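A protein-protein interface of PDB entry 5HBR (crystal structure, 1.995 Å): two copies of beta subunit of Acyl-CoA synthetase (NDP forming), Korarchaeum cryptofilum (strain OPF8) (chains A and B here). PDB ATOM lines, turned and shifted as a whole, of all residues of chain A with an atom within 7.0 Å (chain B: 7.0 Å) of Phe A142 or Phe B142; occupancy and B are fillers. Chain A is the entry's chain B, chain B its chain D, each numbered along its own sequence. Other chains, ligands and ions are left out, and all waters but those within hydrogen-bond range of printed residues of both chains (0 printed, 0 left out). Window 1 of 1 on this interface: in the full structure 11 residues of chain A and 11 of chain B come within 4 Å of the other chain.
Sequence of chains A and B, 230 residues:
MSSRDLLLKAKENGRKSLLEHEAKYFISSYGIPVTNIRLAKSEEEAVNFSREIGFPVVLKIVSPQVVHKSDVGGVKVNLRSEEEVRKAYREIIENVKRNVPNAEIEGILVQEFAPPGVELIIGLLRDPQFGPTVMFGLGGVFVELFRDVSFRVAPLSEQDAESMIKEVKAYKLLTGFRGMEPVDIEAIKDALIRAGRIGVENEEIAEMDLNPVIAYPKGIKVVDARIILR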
ATOM      1  N   GLU A 119      32.371  25.605  18.519  1.00  0.00           N
ATOM      2  CA  GLU A 119      31.683  26.625  19.298  1.00  0.00           C
ATOM      3  C   GLU A 119      30.211  26.728  18.927  1.00  0.00           C
ATOM      4  O   GLU A 119      29.886  26.776  17.741  1.00  0.00           O
ATOM      5  CB  GLU A 119      32.325  27.989  19.094  1.00  0.00           C
ATOM      6  CG  GLU A 119      33.649  28.182  19.799  1.00  0.00           C
ATOM      7  CD  GLU A 119      34.041  29.654  19.886  1.00  0.00           C
ATOM      8  OE1 GLU A 119      33.257  30.520  19.420  1.00  0.00           O
ATOM      9  OE2 GLU A 119      35.128  29.946  20.431  1.00  0.00           O
ATOM     10  N   GLY A 137      22.536  28.326  17.658  1.00  0.00           N
ATOM     11  CA  GLY A 137      23.346  28.656  16.509  1.00  0.00           C
ATOM     12  C   GLY A 137      24.763  28.139  16.682  1.00  0.00           C
ATOM     13  O   GLY A 137      25.177  27.810  17.794  1.00  0.00           O
ATOM     14  N   LEU A 138      25.486  28.020  15.569  1.00  0.00           N
ATOM     15  CA  LEU A 138      26.916  27.761  15.601  1.00  0.00           C
ATOM     16  C   LEU A 138      27.667  29.061  15.910  1.00  0.00           C
ATOM     17  O   LEU A 138      27.254  30.144  15.482  1.00  0.00           O
ATOM     18  CB  LEU A 138      27.379  27.170  14.270  1.00  0.00           C
ATOM     19  CG  LEU A 138      27.296  25.650  14.136  1.00  0.00           C
ATOM     20  CD1 LEU A 138      28.370  24.985  14.974  1.00  0.00           C
ATOM     21  CD2 LEU A 138      25.941  25.121  14.526  1.00  0.00           C
ATOM     22  N   GLY A 139      28.764  28.951  16.652  1.00  0.00           N
ATOM     23  CA  GLY A 139      29.502  30.108  17.117  1.00  0.00           C
ATOM     24  C   GLY A 139      30.296  30.825  16.048  1.00  0.00           C
ATOM     25  O   GLY A 139      30.244  30.474  14.876  1.00  0.00           O
ATOM     26  N   GLY A 140      31.033  31.849  16.459  1.00  0.00           N
ATOM     27  CA  GLY A 140      31.835  32.634  15.536  1.00  0.00           C
ATOM     28  C   GLY A 140      30.991  33.427  14.554  1.00  0.00           C
ATOM     29  O   GLY A 140      30.018  34.074  14.933  1.00  0.00           O
ATOM     30  N   VAL A 141      31.351  33.341  13.278  1.00  0.00           N
ATOM     31  CA  VAL A 141      30.710  34.132  12.233  1.00  0.00           C
ATOM     32  C   VAL A 141      29.311  33.664  11.871  1.00  0.00           C
ATOM     33  O   VAL A 141      28.534  34.411  11.277  1.00  0.00           O
ATOM     34  CB  VAL A 141      31.543  34.118  10.948  1.00  0.00           C
ATOM     35  CG1 VAL A 141      32.881  34.780  11.193  1.00  0.00           C
ATOM     36  CG2 VAL A 141      31.731  32.686  10.434  1.00  0.00           C
ATOM     37  N   PHE A 142      28.983  32.430  12.218  1.00  0.00           N
ATOM     38  CA  PHE A 142      27.740  31.845  11.754  1.00  0.00           C
ATOM     39  C   PHE A 142      26.505  32.496  12.374  1.00  0.00           C
ATOM     40  O   PHE A 142      25.483  32.620  11.699  1.00  0.00           O
ATOM     41  CB  PHE A 142      27.765  30.344  12.001  1.00  0.00           C
ATOM     42  CG  PHE A 142      28.797  29.644  11.175  1.00  0.00           C
ATOM     43  CD1 PHE A 142      28.580  29.413   9.819  1.00  0.00           C
ATOM     44  CD2 PHE A 142      30.003  29.267  11.726  1.00  0.00           C
ATOM     45  CE1 PHE A 142      29.532  28.793   9.052  1.00  0.00           C
ATOM     46  CE2 PHE A 142      30.967  28.642  10.955  1.00  0.00           C
ATOM     47  CZ  PHE A 142      30.731  28.406   9.617  1.00  0.00           C
ATOM     48  N   VAL A 143      26.598  32.942  13.623  1.00  0.00           N
ATOM     49  CA  VAL A 143      25.512  33.700  14.234  1.00  0.00           C
ATOM     50  C   VAL A 143      25.787  35.197  14.103  1.00  0.00           C
ATOM     51  O   VAL A 143      24.920  35.968  13.694  1.00  0.00           O
ATOM     52  CB  VAL A 143      25.321  33.324  15.723  1.00  0.00           C
ATOM     53  CG1 VAL A 143      24.518  34.389  16.472  1.00  0.00           C
ATOM     54  CG2 VAL A 143      24.629  31.973  15.829  1.00  0.00           C
ATOM     55  N   GLU A 144      27.012  35.585  14.430  1.00  0.00           N
ATOM     56  CA  GLU A 144      27.397  36.979  14.514  1.00  0.00           C
ATOM     57  C   GLU A 144      27.334  37.692  13.166  1.00  0.00           C
ATOM     58  O   GLU A 144      26.941  38.850  13.100  1.00  0.00           O
ATOM     59  CB  GLU A 144      28.811  37.078  15.093  1.00  0.00           C
ATOM     60  CG  GLU A 144      29.130  38.409  15.738  1.00  0.00           C
ATOM     61  CD  GLU A 144      30.465  38.404  16.471  1.00  0.00           C
ATOM     62  OE1 GLU A 144      30.945  39.503  16.833  1.00  0.00           O
ATOM     63  OE2 GLU A 144      31.031  37.307  16.696  1.00  0.00           O
ATOM     64  N   LEU A 145      27.717  37.007  12.092  1.00  0.00           N
ATOM     65  CA  LEU A 145      27.762  37.630  10.762  1.00  0.00           C
ATOM     66  C   LEU A 145      26.601  37.188   9.872  1.00  0.00           C
ATOM     67  O   LEU A 145      25.935  38.020   9.253  1.00  0.00           O
ATOM     68  CB  LEU A 145      29.094  37.312  10.074  1.00  0.00           C
ATOM     69  CG  LEU A 145      29.358  38.047   8.756  1.00  0.00           C
ATOM     70  CD1 LEU A 145      29.436  39.549   8.977  1.00  0.00           C
ATOM     71  CD2 LEU A 145      30.631  37.531   8.109  1.00  0.00           C
ATOM     72  N   PHE A 146      26.347  35.886   9.821  1.00  0.00           N
ATOM     73  CA  PHE A 146      25.329  35.334   8.917  1.00  0.00           C
ATOM     74  C   PHE A 146      23.952  35.194   9.567  1.00  0.00           C
ATOM     75  O   PHE A 146      22.976  34.915   8.878  1.00  0.00           O
ATOM     76  CB  PHE A 146      25.752  33.954   8.400  1.00  0.00           C
ATOM     77  CG  PHE A 146      27.046  33.947   7.657  1.00  0.00           C
ATOM     78  CD1 PHE A 146      27.286  34.853   6.645  1.00  0.00           C
ATOM     79  CD2 PHE A 146      28.036  33.025   7.975  1.00  0.00           C
ATOM     80  CE1 PHE A 146      28.488  34.847   5.957  1.00  0.00           C
ATOM     81  CE2 PHE A 146      29.239  33.008   7.290  1.00  0.00           C
ATOM     82  CZ  PHE A 146      29.472  33.919   6.285  1.00  0.00           C
ATOM     83  N   ARG A 147      23.896  35.360  10.888  1.00  0.00           N
ATOM     84  CA  ARG A 147      22.672  35.185  11.675  1.00  0.00           C
ATOM     85  C   ARG A 147      21.927  33.905  11.305  1.00  0.00           C
ATOM     86  O   ARG A 147      20.726  33.903  11.064  1.00  0.00           O
ATOM     87  CB  ARG A 147      21.754  36.415  11.531  1.00  0.00           C
ATOM     88  CG  ARG A 147      22.167  37.626  12.406  1.00  0.00           C
ATOM     89  CD  ARG A 147      22.093  37.337  13.937  1.00  0.00           C
ATOM     90  NE  ARG A 147      20.744  37.449  14.505  1.00  0.00           N
ATOM     91  CZ  ARG A 147      20.436  37.191  15.779  1.00  0.00           C
ATOM     92  NH1 ARG A 147      19.188  37.323  16.210  1.00  0.00           N
ATOM     93  NH2 ARG A 147      21.377  36.801  16.628  1.00  0.00           N
ATOM     94  N   ASP A 148      22.670  32.812  11.297  1.00  0.00           N
ATOM     95  CA  ASP A 148      22.121  31.486  11.080  1.00  0.00           C
ATOM     96  C   ASP A 148      21.682  30.889  12.411  1.00  0.00           C
ATOM     97  O   ASP A 148      22.476  30.244  13.102  1.00  0.00           O
ATOM     98  CB  ASP A 148      23.167  30.597  10.417  1.00  0.00           C
ATOM     99  CG  ASP A 148      22.697  29.174  10.231  1.00  0.00           C
ATOM    100  OD1 ASP A 148      21.483  28.954   9.986  1.00  0.00           O
ATOM    101  OD2 ASP A 148      23.557  28.268  10.326  1.00  0.00           O
ATOM    102  N   VAL A 149      20.431  31.137  12.783  1.00  0.00           N
ATOM    103  CA  VAL A 149      19.918  30.697  14.070  1.00  0.00           C
ATOM    104  C   VAL A 149      18.570  30.005  13.926  1.00  0.00           C
ATOM    105  O   VAL A 149      17.824  30.243  12.981  1.00  0.00           O
ATOM    106  CB  VAL A 149      19.770  31.880  15.058  1.00  0.00           C
ATOM    107  CG1 VAL A 149      21.118  32.417  15.449  1.00  0.00           C
ATOM    108  CG2 VAL A 149      18.927  32.971  14.457  1.00  0.00           C
ATOM    109  N   LYS A 169      21.723  26.277   9.087  1.00  0.00           N
ATOM    110  CA  LYS A 169      22.450  25.980   7.852  1.00  0.00           C
ATOM    111  C   LYS A 169      23.849  25.433   8.127  1.00  0.00           C
ATOM    112  O   LYS A 169      24.415  24.738   7.287  1.00  0.00           O
ATOM    113  CB  LYS A 169      22.524  27.223   6.966  1.00  0.00           C
ATOM    114  CG  LYS A 169      21.254  27.447   6.143  1.00  0.00           C
ATOM    115  CD  LYS A 169      21.007  28.909   5.819  1.00  0.00           C
ATOM    116  CE  LYS A 169      20.819  29.734   7.092  1.00  0.00           C
ATOM    117  NZ  LYS A 169      19.967  30.942   6.896  1.00  0.00           N
ATOM    118  N   ALA A 170      24.392  25.723   9.306  1.00  0.00           N
ATOM    119  CA  ALA A 170      25.751  25.298   9.651  1.00  0.00           C
ATOM    120  C   ALA A 170      25.774  23.966  10.390  1.00  0.00           C
ATOM    121  O   ALA A 170      26.754  23.640  11.048  1.00  0.00           O
ATOM    122  CB  ALA A 170      26.432  26.358  10.488  1.00  0.00           C
ATOM    123  N   LEU A 173      28.728  21.238  10.646  1.00  0.00           N
ATOM    124  CA  LEU A 173      29.868  21.449  11.523  1.00  0.00           C
ATOM    125  C   LEU A 173      29.756  20.582  12.774  1.00  0.00           C
ATOM    126  O   LEU A 173      30.730  20.424  13.503  1.00  0.00           O
ATOM    127  CB  LEU A 173      29.988  22.920  11.925  1.00  0.00           C
ATOM    128  CG  LEU A 173      30.389  23.895  10.824  1.00  0.00           C
ATOM    129  CD1 LEU A 173      30.443  25.300  11.371  1.00  0.00           C
ATOM    130  CD2 LEU A 173      31.723  23.520  10.219  1.00  0.00           C
ATOM    131  N   GLU B 119      40.633  33.110   2.759  1.00  0.00           N
ATOM    132  CA  GLU B 119      40.912  32.108   1.737  1.00  0.00           C
ATOM    133  C   GLU B 119      39.754  31.953   0.754  1.00  0.00           C
ATOM    134  O   GLU B 119      38.590  32.056   1.134  1.00  0.00           O
ATOM    135  CB  GLU B 119      41.205  30.752   2.374  1.00  0.00           C
ATOM    136  CG  GLU B 119      42.568  30.670   3.038  1.00  0.00           C
ATOM    137  CD  GLU B 119      42.922  29.267   3.479  1.00  0.00           C
ATOM    138  OE1 GLU B 119      42.049  28.375   3.406  1.00  0.00           O
ATOM    139  OE2 GLU B 119      44.082  29.051   3.883  1.00  0.00           O
ATOM    140  N   GLY B 137      34.187  30.472  -4.743  1.00  0.00           N
ATOM    141  CA  GLY B 137      33.645  30.193  -3.434  1.00  0.00           C
ATOM    142  C   GLY B 137      34.675  30.534  -2.392  1.00  0.00           C
ATOM    143  O   GLY B 137      35.858  30.683  -2.704  1.00  0.00           O
ATOM    144  N   LEU B 138      34.237  30.653  -1.146  1.00  0.00           N
ATOM    145  CA  LEU B 138      35.175  30.868  -0.058  1.00  0.00           C
ATOM    146  C   LEU B 138      35.778  29.549   0.402  1.00  0.00           C
ATOM    147  O   LEU B 138      35.161  28.487   0.285  1.00  0.00           O
ATOM    148  CB  LEU B 138      34.487  31.609   1.084  1.00  0.00           C
ATOM    149  CG  LEU B 138      34.551  33.103   0.739  1.00  0.00           C
ATOM    150  CD1 LEU B 138      33.205  33.641   0.307  1.00  0.00           C
ATOM    151  CD2 LEU B 138      35.136  33.881   1.885  1.00  0.00           C
ATOM    152  N   GLY B 139      37.007  29.628   0.902  1.00  0.00           N
ATOM    153  CA  GLY B 139      37.805  28.456   1.184  1.00  0.00           C
ATOM    154  C   GLY B 139      37.347  27.745   2.435  1.00  0.00           C
ATOM    155  O   GLY B 139      36.354  28.128   3.050  1.00  0.00           O
ATOM    156  N   GLY B 140      38.065  26.691   2.799  1.00  0.00           N
ATOM    157  CA  GLY B 140      37.759  25.938   3.995  1.00  0.00           C
ATOM    158  C   GLY B 140      36.440  25.205   3.892  1.00  0.00           C
ATOM    159  O   GLY B 140      36.128  24.599   2.873  1.00  0.00           O
ATOM    160  N   VAL B 141      35.652  25.277   4.956  1.00  0.00           N
ATOM    161  CA  VAL B 141      34.435  24.495   5.048  1.00  0.00           C
ATOM    162  C   VAL B 141      33.343  24.982   4.102  1.00  0.00           C
ATOM    163  O   VAL B 141      32.374  24.275   3.858  1.00  0.00           O
ATOM    164  CB  VAL B 141      33.890  24.501   6.489  1.00  0.00           C
ATOM    165  CG1 VAL B 141      34.887  23.826   7.423  1.00  0.00           C
ATOM    166  CG2 VAL B 141      33.580  25.930   6.950  1.00  0.00           C
ATOM    167  N   PHE B 142      33.499  26.176   3.558  1.00  0.00           N
ATOM    168  CA  PHE B 142      32.399  26.803   2.825  1.00  0.00           C
ATOM    169  C   PHE B 142      32.194  26.172   1.443  1.00  0.00           C
ATOM    170  O   PHE B 142      31.065  26.011   0.995  1.00  0.00           O
ATOM    171  CB  PHE B 142      32.640  28.307   2.727  1.00  0.00           C
ATOM    172  CG  PHE B 142      32.583  28.990   4.061  1.00  0.00           C
ATOM    173  CD1 PHE B 142      31.363  29.336   4.623  1.00  0.00           C
ATOM    174  CD2 PHE B 142      33.745  29.239   4.779  1.00  0.00           C
ATOM    175  CE1 PHE B 142      31.302  29.941   5.869  1.00  0.00           C
ATOM    176  CE2 PHE B 142      33.699  29.842   6.026  1.00  0.00           C
ATOM    177  CZ  PHE B 142      32.480  30.192   6.575  1.00  0.00           C
ATOM    178  N   VAL B 143      33.281  25.787   0.793  1.00  0.00           N
ATOM    179  CA  VAL B 143      33.184  25.049  -0.453  1.00  0.00           C
ATOM    180  C   VAL B 143      33.166  23.561  -0.133  1.00  0.00           C
ATOM    181  O   VAL B 143      32.351  22.795  -0.654  1.00  0.00           O
ATOM    182  CB  VAL B 143      34.356  25.378  -1.400  1.00  0.00           C
ATOM    183  CG1 VAL B 143      35.710  25.183  -0.678  1.00  0.00           C
ATOM    184  CG2 VAL B 143      34.293  24.526  -2.657  1.00  0.00           C
ATOM    185  N   GLU B 144      34.056  23.172   0.770  1.00  0.00           N
ATOM    186  CA  GLU B 144      34.399  21.777   0.979  1.00  0.00           C
ATOM    187  C   GLU B 144      33.259  21.016   1.630  1.00  0.00           C
ATOM    188  O   GLU B 144      33.003  19.864   1.292  1.00  0.00           O
ATOM    189  CB  GLU B 144      35.657  21.702   1.845  1.00  0.00           C
ATOM    190  CG  GLU B 144      36.465  20.439   1.717  1.00  0.00           C
ATOM    191  CD  GLU B 144      37.750  20.512   2.532  1.00  0.00           C
ATOM    192  OE1 GLU B 144      38.408  21.580   2.524  1.00  0.00           O
ATOM    193  OE2 GLU B 144      38.092  19.507   3.191  1.00  0.00           O
ATOM    194  N   LEU B 145      32.574  21.685   2.556  1.00  0.00           N
ATOM    195  CA  LEU B 145      31.523  21.074   3.358  1.00  0.00           C
ATOM    196  C   LEU B 145      30.131  21.561   2.944  1.00  0.00           C
ATOM    197  O   LEU B 145      29.231  20.754   2.705  1.00  0.00           O
ATOM    198  CB  LEU B 145      31.775  21.373   4.840  1.00  0.00           C
ATOM    199  CG  LEU B 145      31.060  20.512   5.876  1.00  0.00           C
ATOM    200  CD1 LEU B 145      31.653  19.122   5.928  1.00  0.00           C
ATOM    201  CD2 LEU B 145      31.142  21.170   7.233  1.00  0.00           C
ATOM    202  N   PHE B 146      29.947  22.879   2.861  1.00  0.00           N
ATOM    203  CA  PHE B 146      28.622  23.449   2.575  1.00  0.00           C
ATOM    204  C   PHE B 146      28.315  23.578   1.079  1.00  0.00           C
ATOM    205  O   PHE B 146      27.182  23.884   0.716  1.00  0.00           O
ATOM    206  CB  PHE B 146      28.476  24.833   3.211  1.00  0.00           C
ATOM    207  CG  PHE B 146      28.617  24.835   4.693  1.00  0.00           C
ATOM    208  CD1 PHE B 146      27.790  24.062   5.477  1.00  0.00           C
ATOM    209  CD2 PHE B 146      29.584  25.613   5.303  1.00  0.00           C
ATOM    210  CE1 PHE B 146      27.935  24.054   6.843  1.00  0.00           C
ATOM    211  CE2 PHE B 146      29.729  25.612   6.667  1.00  0.00           C
ATOM    212  CZ  PHE B 146      28.904  24.842   7.441  1.00  0.00           C
ATOM    213  N   ARG B 147      29.322  23.369   0.227  1.00  0.00           N
ATOM    214  CA  ARG B 147      29.156  23.455  -1.235  1.00  0.00           C
ATOM    215  C   ARG B 147      28.573  24.797  -1.699  1.00  0.00           C
ATOM    216  O   ARG B 147      27.736  24.834  -2.613  1.00  0.00           O
ATOM    217  CB  ARG B 147      28.255  22.316  -1.742  1.00  0.00           C
ATOM    218  CG  ARG B 147      28.699  20.912  -1.363  1.00  0.00           C
ATOM    219  CD  ARG B 147      30.197  20.746  -1.542  1.00  0.00           C
ATOM    220  NE  ARG B 147      30.578  19.430  -2.035  1.00  0.00           N
ATOM    221  CZ  ARG B 147      31.830  19.077  -2.315  1.00  0.00           C
ATOM    222  NH1 ARG B 147      32.829  19.939  -2.140  1.00  0.00           N
ATOM    223  NH2 ARG B 147      32.086  17.857  -2.768  1.00  0.00           N
ATOM    224  N   ASP B 148      29.021  25.882  -1.063  1.00  0.00           N
ATOM    225  CA  ASP B 148      28.561  27.235  -1.358  1.00  0.00           C
ATOM    226  C   ASP B 148      29.407  27.878  -2.462  1.00  0.00           C
ATOM    227  O   ASP B 148      30.390  28.569  -2.187  1.00  0.00           O
ATOM    228  CB  ASP B 148      28.607  28.085  -0.075  1.00  0.00           C
ATOM    229  CG  ASP B 148      28.326  29.558  -0.321  1.00  0.00           C
ATOM    230  OD1 ASP B 148      27.442  29.887  -1.144  1.00  0.00           O
ATOM    231  OD2 ASP B 148      28.999  30.397   0.326  1.00  0.00           O
ATOM    232  N   VAL B 149      29.033  27.634  -3.711  1.00  0.00           N
ATOM    233  CA  VAL B 149      29.820  28.090  -4.850  1.00  0.00           C
ATOM    234  C   VAL B 149      28.946  28.718  -5.915  1.00  0.00           C
ATOM    235  O   VAL B 149      27.752  28.434  -6.001  1.00  0.00           O
ATOM    236  CB  VAL B 149      30.608  26.947  -5.486  1.00  0.00           C
ATOM    237  CG1 VAL B 149      31.625  26.388  -4.504  1.00  0.00           C
ATOM    238  CG2 VAL B 149      29.684  25.862  -5.948  1.00  0.00           C
ATOM    239  N   LYS B 169      26.753  32.554  -0.517  1.00  0.00           N
ATOM    240  CA  LYS B 169      26.230  32.837   0.817  1.00  0.00           C
ATOM    241  C   LYS B 169      27.287  33.384   1.766  1.00  0.00           C
ATOM    242  O   LYS B 169      26.988  34.205   2.627  1.00  0.00           O
ATOM    243  CB  LYS B 169      25.606  31.576   1.421  1.00  0.00           C
ATOM    244  CG  LYS B 169      24.094  31.515   1.243  1.00  0.00           C
ATOM    245  CD  LYS B 169      23.689  30.611   0.109  1.00  0.00           C
ATOM    246  CE  LYS B 169      23.601  29.157   0.558  1.00  0.00           C
ATOM    247  NZ  LYS B 169      22.493  28.436  -0.137  1.00  0.00           N
ATOM    248  N   ALA B 170      28.526  32.949   1.603  1.00  0.00           N
ATOM    249  CA  ALA B 170      29.596  33.403   2.497  1.00  0.00           C
ATOM    250  C   ALA B 170      30.191  34.741   2.053  1.00  0.00           C
ATOM    251  O   ALA B 170      31.250  35.117   2.522  1.00  0.00           O
ATOM    252  CB  ALA B 170      30.700  32.334   2.587  1.00  0.00           C
ATOM    253  N   LEU B 173      32.065  37.451   4.186  1.00  0.00           N
ATOM    254  CA  LEU B 173      33.422  37.204   4.659  1.00  0.00           C
ATOM    255  C   LEU B 173      34.437  38.048   3.891  1.00  0.00           C
ATOM    256  O   LEU B 173      35.611  38.088   4.250  1.00  0.00           O
ATOM    257  CB  LEU B 173      33.782  35.722   4.535  1.00  0.00           C
ATOM    258  CG  LEU B 173      33.139  34.751   5.527  1.00  0.00           C
ATOM    259  CD1 LEU B 173      33.706  33.346   5.343  1.00  0.00           C
ATOM    260  CD2 LEU B 173      33.320  35.204   6.982  1.00  0.00           C
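Phe B142 touches its own counterpart, Phe A142. Leu A145 touches Leu B173, and with the chains exchanged Leu A173 touches Leu B145. Phe A146 touches Lys B169, and with the chains exchanged Lys A169 touches Phe B146. Phe A146 touches Leu B173, and with the chains exchanged Leu A173 touches Phe B146. Of the 11 pairs that touch across the chains among the printed residues, 11 have their exchanged pair printed and touching as well.
Among the printed residues, pairs that only touch across the chains: Phe A142 with Phe B142 (3.8 Å), Phe A142 with Phe B146 (3.98 Å), Leu A145 with Leu B173 (3.7 Å), Phe A146 with Phe B142 (3.96 Å), Phe A146 with Lys B169 (3.7 Å), Phe A146 with Ala B170 (3.8 Å), Phe A146 with Leu B173 (3.8 Å), Lys A169 with Phe B146 (3.6 Å), Ala A170 with Phe B146 (3.8 Å), Leu A173 with Leu B145 (3.8 Å) and Leu A173 with Phe B146 (3.8 Å).
Printed residues of chain A that touch a printed residue of chain B: Phe A142, Leu A145, Phe A146, Lys A169, Ala A170 and Leu A173. Along chain B the printed residues that touch a printed residue of chain A span positions 142 to 173. Among the printed residues, 11 pairs touch across the chains. Among the printed residues, no Asp or Glu carboxylate lies within 4 Å of a Lys or Arg side-chain nitrogen of the other chain.
O of Phe A142 lies within hydrogen-bond range of N of Arg A147 (3.3 Å). NZ of Lys A169 lies within salt-bridge range of OD1 of Asp A148 (3.97 Å). OD2 of Asp A148 lies within hydrogen-bond range of N of Ala A170 (2.9 Å). The backbone NH (N) of Arg B147 is in hydrogen-bond range of the backbone carbonyl oxygen (O) of Phe B142. N of Asp B148 is in hydrogen-bond range of O of Phe B142, 2.9 Å away. The side-chain carboxylate (OD2) of Asp B148 sits at hydrogen-bond distance from the backbone NH (N) of Ala B170.
Of the printed residues of chain B, Phe A142 touches Phe B142 (3.8 Å) and Phe B146 (3.98 Å). Printed residues of chain B within 4 Å of Leu A145: Leu B173. Of the printed residues of chain B, Lys A169 touches Phe B146. Printed residues of chain B within 4 Å of Ala A170: Phe B146 (3.8 Å). Gly B139 touches none of the printed residues of chain A. Phe B142 touches just these residues of chain A: Phe A142 (3.8 Å) and Phe A146 (3.96 Å). Of the printed residues of chain A, Phe B146 touches Phe A142 (3.98 Å), Lys A169 (3.6 Å), Ala A170 (3.8 Å) and Leu A173 (3.8 Å). Val B149 touches none of the printed residues of chain A. The nearest printed residue of chain B that does not touch Phe A142 is Val B141 (4.6 Å).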
